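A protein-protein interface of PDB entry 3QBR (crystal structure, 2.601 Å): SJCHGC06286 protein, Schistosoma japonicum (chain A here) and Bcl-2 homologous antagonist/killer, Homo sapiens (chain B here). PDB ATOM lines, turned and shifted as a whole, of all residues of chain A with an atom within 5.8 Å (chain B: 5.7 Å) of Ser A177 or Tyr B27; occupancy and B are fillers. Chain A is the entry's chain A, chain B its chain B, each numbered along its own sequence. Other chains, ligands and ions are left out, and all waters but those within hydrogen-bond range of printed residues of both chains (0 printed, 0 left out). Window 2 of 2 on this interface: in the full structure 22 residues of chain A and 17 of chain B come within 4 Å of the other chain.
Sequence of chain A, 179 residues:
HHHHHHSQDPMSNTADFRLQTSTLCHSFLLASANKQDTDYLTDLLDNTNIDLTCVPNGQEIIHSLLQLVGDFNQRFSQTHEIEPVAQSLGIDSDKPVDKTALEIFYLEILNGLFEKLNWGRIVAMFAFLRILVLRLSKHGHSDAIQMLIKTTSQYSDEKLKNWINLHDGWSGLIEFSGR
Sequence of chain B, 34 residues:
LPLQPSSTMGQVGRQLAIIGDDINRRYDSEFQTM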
ATOM      1  N   SER A  64      15.307   1.252 -16.684  1.00  0.00           N
ATOM      2  CA  SER A  64      14.152   2.114 -16.827  1.00  0.00           C
ATOM      3  C   SER A  64      12.972   1.495 -16.130  1.00  0.00           C
ATOM      4  O   SER A  64      12.273   2.169 -15.382  1.00  0.00           O
ATOM      5  CB  SER A  64      13.807   2.344 -18.299  1.00  0.00           C
ATOM      6  OG  SER A  64      14.738   3.227 -18.887  1.00  0.00           O
ATOM      7  N   GLN A  67      13.106   1.783 -12.379  1.00  0.00           N
ATOM      8  CA  GLN A  67      12.751   3.121 -11.959  1.00  0.00           C
ATOM      9  C   GLN A  67      11.230   3.342 -12.042  1.00  0.00           C
ATOM     10  O   GLN A  67      10.619   3.799 -11.086  1.00  0.00           O
ATOM     11  CB  GLN A  67      13.507   4.144 -12.775  1.00  0.00           C
ATOM     12  CG  GLN A  67      13.139   5.581 -12.428  1.00  0.00           C
ATOM     13  CD  GLN A  67      13.542   6.521 -13.538  1.00  0.00           C
ATOM     14  OE1 GLN A  67      14.729   6.744 -13.760  1.00  0.00           O
ATOM     15  NE2 GLN A  67      12.554   7.042 -14.277  1.00  0.00           N
ATOM     16  N   LEU A  68      10.634   2.954 -13.166  1.00  0.00           N
ATOM     17  CA  LEU A  68       9.233   3.225 -13.473  1.00  0.00           C
ATOM     18  C   LEU A  68       8.247   2.337 -12.711  1.00  0.00           C
ATOM     19  O   LEU A  68       7.146   2.775 -12.400  1.00  0.00           O
ATOM     20  CB  LEU A  68       8.988   3.091 -14.986  1.00  0.00           C
ATOM     21  CG  LEU A  68       9.634   4.112 -15.933  1.00  0.00           C
ATOM     22  CD1 LEU A  68       9.521   3.648 -17.386  1.00  0.00           C
ATOM     23  CD2 LEU A  68       9.027   5.489 -15.787  1.00  0.00           C
ATOM     24  N   ASP A  71       8.137   3.950  -9.453  1.00  0.00           N
ATOM     25  CA  ASP A  71       7.141   5.012  -9.473  1.00  0.00           C
ATOM     26  C   ASP A  71       5.794   4.392  -9.205  1.00  0.00           C
ATOM     27  O   ASP A  71       5.035   4.882  -8.366  1.00  0.00           O
ATOM     28  CB  ASP A  71       7.107   5.723 -10.826  1.00  0.00           C
ATOM     29  CG  ASP A  71       8.329   6.612 -11.069  1.00  0.00           C
ATOM     30  OD1 ASP A  71       8.949   7.095 -10.091  1.00  0.00           O
ATOM     31  OD2 ASP A  71       8.656   6.840 -12.257  1.00  0.00           O
ATOM     32  N   ARG A  75       3.167   4.694  -5.613  1.00  0.00           N
ATOM     33  CA  ARG A  75       1.785   5.199  -5.717  1.00  0.00           C
ATOM     34  C   ARG A  75       0.696   4.186  -5.338  1.00  0.00           C
ATOM     35  O   ARG A  75      -0.341   4.565  -4.816  1.00  0.00           O
ATOM     36  CB  ARG A  75       1.491   5.756  -7.128  1.00  0.00           C
ATOM     37  CG  ARG A  75       2.355   6.945  -7.489  1.00  0.00           C
ATOM     38  CD  ARG A  75       2.361   7.272  -8.987  1.00  0.00           C
ATOM     39  NE  ARG A  75       3.583   7.995  -9.360  1.00  0.00           N
ATOM     40  CZ  ARG A  75       3.682   8.882 -10.349  1.00  0.00           C
ATOM     41  NH1 ARG A  75       2.621   9.195 -11.076  1.00  0.00           N
ATOM     42  NH2 ARG A  75       4.844   9.475 -10.598  1.00  0.00           N
ATOM     43  N   GLY A 172      11.751   2.198 -26.305  1.00  0.00           N
ATOM     44  CA  GLY A 172      10.956   3.382 -26.025  1.00  0.00           C
ATOM     45  C   GLY A 172      11.038   3.734 -24.553  1.00  0.00           C
ATOM     46  O   GLY A 172      11.171   4.908 -24.167  1.00  0.00           O
ATOM     47  N   LEU A 173      10.989   2.694 -23.728  1.00  0.00           N
ATOM     48  CA  LEU A 173      11.015   2.851 -22.280  1.00  0.00           C
ATOM     49  C   LEU A 173      12.209   3.703 -21.799  1.00  0.00           C
ATOM     50  O   LEU A 173      12.095   4.503 -20.863  1.00  0.00           O
ATOM     51  CB  LEU A 173      11.001   1.465 -21.612  1.00  0.00           C
ATOM     52  CG  LEU A 173       9.698   0.684 -21.780  1.00  0.00           C
ATOM     53  CD1 LEU A 173       9.940  -0.796 -21.567  1.00  0.00           C
ATOM     54  CD2 LEU A 173       8.584   1.224 -20.845  1.00  0.00           C
ATOM     55  N   ILE A 174      13.353   3.521 -22.441  1.00  0.00           N
ATOM     56  CA  ILE A 174      14.553   4.213 -22.013  1.00  0.00           C
ATOM     57  C   ILE A 174      14.295   5.719 -22.035  1.00  0.00           C
ATOM     58  O   ILE A 174      14.361   6.396 -21.005  1.00  0.00           O
ATOM     59  CB  ILE A 174      15.744   3.838 -22.893  1.00  0.00           C
ATOM     60  CG1 ILE A 174      16.036   2.339 -22.747  1.00  0.00           C
ATOM     61  CG2 ILE A 174      16.949   4.679 -22.518  1.00  0.00           C
ATOM     62  CD1 ILE A 174      17.086   1.821 -23.690  1.00  0.00           C
ATOM     63  N   GLU A 175      13.952   6.234 -23.207  1.00  0.00           N
ATOM     64  CA  GLU A 175      13.620   7.644 -23.345  1.00  0.00           C
ATOM     65  C   GLU A 175      12.370   8.035 -22.550  1.00  0.00           C
ATOM     66  O   GLU A 175      12.366   9.055 -21.881  1.00  0.00           O
ATOM     67  CB  GLU A 175      13.437   7.989 -24.817  1.00  0.00           C
ATOM     68  CG  GLU A 175      13.619   9.455 -25.144  1.00  0.00           C
ATOM     69  CD  GLU A 175      13.656   9.696 -26.652  1.00  0.00           C
ATOM     70  OE1 GLU A 175      13.739  10.870 -27.081  1.00  0.00           O
ATOM     71  OE2 GLU A 175      13.600   8.701 -27.415  1.00  0.00           O
ATOM     72  N   PHE A 176      11.311   7.235 -22.623  1.00  0.00           N
ATOM     73  CA  PHE A 176      10.100   7.544 -21.862  1.00  0.00           C
ATOM     74  C   PHE A 176      10.444   7.972 -20.443  1.00  0.00           C
ATOM     75  O   PHE A 176       9.783   8.831 -19.851  1.00  0.00           O
ATOM     76  CB  PHE A 176       9.164   6.338 -21.811  1.00  0.00           C
ATOM     77  CG  PHE A 176       7.928   6.561 -20.977  1.00  0.00           C
ATOM     78  CD1 PHE A 176       6.988   7.517 -21.338  1.00  0.00           C
ATOM     79  CD2 PHE A 176       7.705   5.815 -19.823  1.00  0.00           C
ATOM     80  CE1 PHE A 176       5.842   7.728 -20.559  1.00  0.00           C
ATOM     81  CE2 PHE A 176       6.554   6.012 -19.045  1.00  0.00           C
ATOM     82  CZ  PHE A 176       5.626   6.976 -19.410  1.00  0.00           C
ATOM     83  N   SER A 177      11.504   7.379 -19.915  1.00  0.00           N
ATOM     84  CA  SER A 177      11.860   7.515 -18.513  1.00  0.00           C
ATOM     85  C   SER A 177      12.900   8.596 -18.218  1.00  0.00           C
ATOM     86  O   SER A 177      13.180   8.843 -17.058  1.00  0.00           O
ATOM     87  CB  SER A 177      12.381   6.175 -17.995  1.00  0.00           C
ATOM     88  OG  SER A 177      13.548   5.802 -18.705  1.00  0.00           O
ATOM     89  N   GLY A 178      13.489   9.199 -19.254  1.00  0.00           N
ATOM     90  CA  GLY A 178      14.532  10.204 -19.088  1.00  0.00           C
ATOM     91  C   GLY A 178      15.941   9.663 -18.888  1.00  0.00           C
ATOM     92  O   GLY A 178      16.379   8.693 -19.528  1.00  0.00           O
ATOM     93  N   ASP B  22      -1.150   8.360 -14.787  1.00  0.00           N
ATOM     94  CA  ASP B  22      -0.402   9.316 -13.962  1.00  0.00           C
ATOM     95  C   ASP B  22       1.089   9.266 -14.289  1.00  0.00           C
ATOM     96  O   ASP B  22       1.749  10.305 -14.425  1.00  0.00           O
ATOM     97  CB  ASP B  22      -0.619   9.073 -12.464  1.00  0.00           C
ATOM     98  CG  ASP B  22      -2.004   9.490 -11.989  1.00  0.00           C
ATOM     99  OD1 ASP B  22      -2.510   8.876 -11.022  1.00  0.00           O
ATOM    100  OD2 ASP B  22      -2.591  10.427 -12.577  1.00  0.00           O
ATOM    101  N   ILE B  23       1.616   8.048 -14.422  1.00  0.00           N
ATOM    102  CA  ILE B  23       3.014   7.859 -14.777  1.00  0.00           C
ATOM    103  C   ILE B  23       3.233   8.464 -16.156  1.00  0.00           C
ATOM    104  O   ILE B  23       4.156   9.251 -16.386  1.00  0.00           O
ATOM    105  CB  ILE B  23       3.391   6.354 -14.740  1.00  0.00           C
ATOM    106  CG1 ILE B  23       3.616   5.910 -13.292  1.00  0.00           C
ATOM    107  CG2 ILE B  23       4.647   6.073 -15.576  1.00  0.00           C
ATOM    108  CD1 ILE B  23       3.338   4.458 -13.058  1.00  0.00           C
ATOM    109  N   ASN B  24       2.340   8.118 -17.064  1.00  0.00           N
ATOM    110  CA  ASN B  24       2.446   8.574 -18.436  1.00  0.00           C
ATOM    111  C   ASN B  24       2.485  10.102 -18.557  1.00  0.00           C
ATOM    112  O   ASN B  24       3.330  10.664 -19.256  1.00  0.00           O
ATOM    113  CB  ASN B  24       1.307   7.980 -19.246  1.00  0.00           C
ATOM    114  CG  ASN B  24       1.402   8.325 -20.699  1.00  0.00           C
ATOM    115  OD1 ASN B  24       0.425   8.770 -21.289  1.00  0.00           O
ATOM    116  ND2 ASN B  24       2.576   8.124 -21.294  1.00  0.00           N
ATOM    117  N   ARG B  25       1.577  10.770 -17.852  1.00  0.00           N
ATOM    118  CA  ARG B  25       1.541  12.230 -17.822  1.00  0.00           C
ATOM    119  C   ARG B  25       2.849  12.840 -17.312  1.00  0.00           C
ATOM    120  O   ARG B  25       3.386  13.772 -17.909  1.00  0.00           O
ATOM    121  CB  ARG B  25       0.367  12.719 -16.962  1.00  0.00           C
ATOM    122  CG  ARG B  25      -0.991  12.628 -17.632  1.00  0.00           C
ATOM    123  CD  ARG B  25      -2.109  12.340 -16.627  1.00  0.00           C
ATOM    124  NE  ARG B  25      -3.287  11.730 -17.265  1.00  0.00           N
ATOM    125  CZ  ARG B  25      -4.306  11.172 -16.609  1.00  0.00           C
ATOM    126  NH1 ARG B  25      -4.314  11.129 -15.278  1.00  0.00           N
ATOM    127  NH2 ARG B  25      -5.323  10.654 -17.286  1.00  0.00           N
ATOM    128  N   ARG B  26       3.355  12.314 -16.206  1.00  0.00           N
ATOM    129  CA  ARG B  26       4.528  12.886 -15.582  1.00  0.00           C
ATOM    130  C   ARG B  26       5.729  12.826 -16.512  1.00  0.00           C
ATOM    131  O   ARG B  26       6.567  13.726 -16.532  1.00  0.00           O
ATOM    132  CB  ARG B  26       4.823  12.145 -14.287  1.00  0.00           C
ATOM    133  CG  ARG B  26       6.244  12.301 -13.760  1.00  0.00           C
ATOM    134  CD  ARG B  26       6.300  11.787 -12.320  1.00  0.00           C
ATOM    135  NE  ARG B  26       7.646  11.482 -11.826  1.00  0.00           N
ATOM    136  CZ  ARG B  26       7.901  11.066 -10.586  1.00  0.00           C
ATOM    137  NH1 ARG B  26       6.904  10.909  -9.721  1.00  0.00           N
ATOM    138  NH2 ARG B  26       9.146  10.811 -10.211  1.00  0.00           N
ATOM    139  N   TYR B  27       5.801  11.760 -17.298  1.00  0.00           N
ATOM    140  CA  TYR B  27       6.991  11.510 -18.091  1.00  0.00           C
ATOM    141  C   TYR B  27       6.921  12.126 -19.476  1.00  0.00           C
ATOM    142  O   TYR B  27       7.866  12.022 -20.261  1.00  0.00           O
ATOM    143  CB  TYR B  27       7.325  10.007 -18.125  1.00  0.00           C
ATOM    144  CG  TYR B  27       8.006   9.582 -16.853  1.00  0.00           C
ATOM    145  CD1 TYR B  27       9.341   9.900 -16.630  1.00  0.00           C
ATOM    146  CD2 TYR B  27       7.307   8.916 -15.845  1.00  0.00           C
ATOM    147  CE1 TYR B  27       9.977   9.541 -15.455  1.00  0.00           C
ATOM    148  CE2 TYR B  27       7.937   8.545 -14.656  1.00  0.00           C
ATOM    149  CZ  TYR B  27       9.273   8.866 -14.470  1.00  0.00           C
ATOM    150  OH  TYR B  27       9.922   8.514 -13.309  1.00  0.00           O
ATOM    151  N   ASP B  28       5.810  12.786 -19.769  1.00  0.00           N
ATOM    152  CA  ASP B  28       5.696  13.533 -21.013  1.00  0.00           C
ATOM    153  C   ASP B  28       6.675  14.718 -21.017  1.00  0.00           C
ATOM    154  O   ASP B  28       6.729  15.484 -20.049  1.00  0.00           O
ATOM    155  CB  ASP B  28       4.264  14.014 -21.205  1.00  0.00           C
ATOM    156  CG  ASP B  28       3.877  14.107 -22.659  1.00  0.00           C
ATOM    157  OD1 ASP B  28       3.131  13.217 -23.119  1.00  0.00           O
ATOM    158  OD2 ASP B  28       4.325  15.056 -23.340  1.00  0.00           O
ATOM    159  N   SER B  29       7.448  14.847 -22.102  1.00  0.00           N
ATOM    160  CA  SER B  29       8.476  15.891 -22.247  1.00  0.00           C
ATOM    161  C   SER B  29       7.963  17.297 -21.961  1.00  0.00           C
ATOM    162  O   SER B  29       8.757  18.221 -21.755  1.00  0.00           O
ATOM    163  CB  SER B  29       9.095  15.865 -23.648  1.00  0.00           C
ATOM    164  OG  SER B  29      10.257  15.056 -23.679  1.00  0.00           O
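NE2 of Gln A67 lies within hydrogen-bond range of OH of Tyr B27, 3.2 Å away.
The guanidinium group of Arg B26 lies within salt-bridge range of the side-chain carboxylate of Asp A71, 3.7 Å away.
The guanidinium group of Arg A75 sits close to the guanidinium group of Arg B26 (2.7 Å).
OH of Tyr B27 lies close to OD2 of Asp A71, 2.3 Å away.
The side-chain hydroxyl of Ser A177 lies within hydrogen-bond range of the side-chain hydroxyl of Ser A64, 2.8 Å away.
NE2 of Gln A67 is in hydrogen-bond range of O of Ser A177 (3.4 Å).
The backbone carbonyl oxygen of Leu A173 lies within hydrogen-bond range of the side-chain hydroxyl of Ser A177, 2.9 Å away.
The side-chain hydroxyl (OG) of Ser A177 lies within hydrogen-bond range of the backbone carbonyl oxygen (O) of Ile A174.
The side-chain carboxylate of Asp B22 lies within salt-bridge range of the guanidinium group of Arg B25 (3.3 Å).
Among the printed residues, pairs that only touch across the chains: Phe A176 with Tyr B27, Phe A176 with Asn B24, Leu A68 with Tyr B27, Arg A75 with Asp B22, Ser A177 with Tyr B27, Arg A75 with Ile B23 and Phe A176 with Ile B23.
Of chain B, only Tyr B27 comes within 4 Å of Ser A177.
Of chain A, only Gln A67 (3.2 Å), Leu A68 (3.4 Å), Asp A71 (2.3 Å), Phe A176 (3.2 Å) and Ser A177 (3.6 Å) come within 4 Å of Tyr B27.
Of the printed residues of chain B, Gln A67 touches Tyr B27 (3.2 Å).
Printed residues of chain B within 4 Å of Phe A176: Ile B23 (3.96 Å), Asn B24 (3.4 Å) and Tyr B27 (3.2 Å).
The nearest printed residue of chain B that does not touch Ser A177 is Asp B28 (7.9 Å).
Printed residues of chain B that touch a printed residue of chain A: Asp B22, Ile B23, Asn B24, Arg B26 and Tyr B27.
Along chain B the printed residues that touch a printed residue of chain A span positions 22 to 27.
Among the printed residues, 11 pairs touch across the chains.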
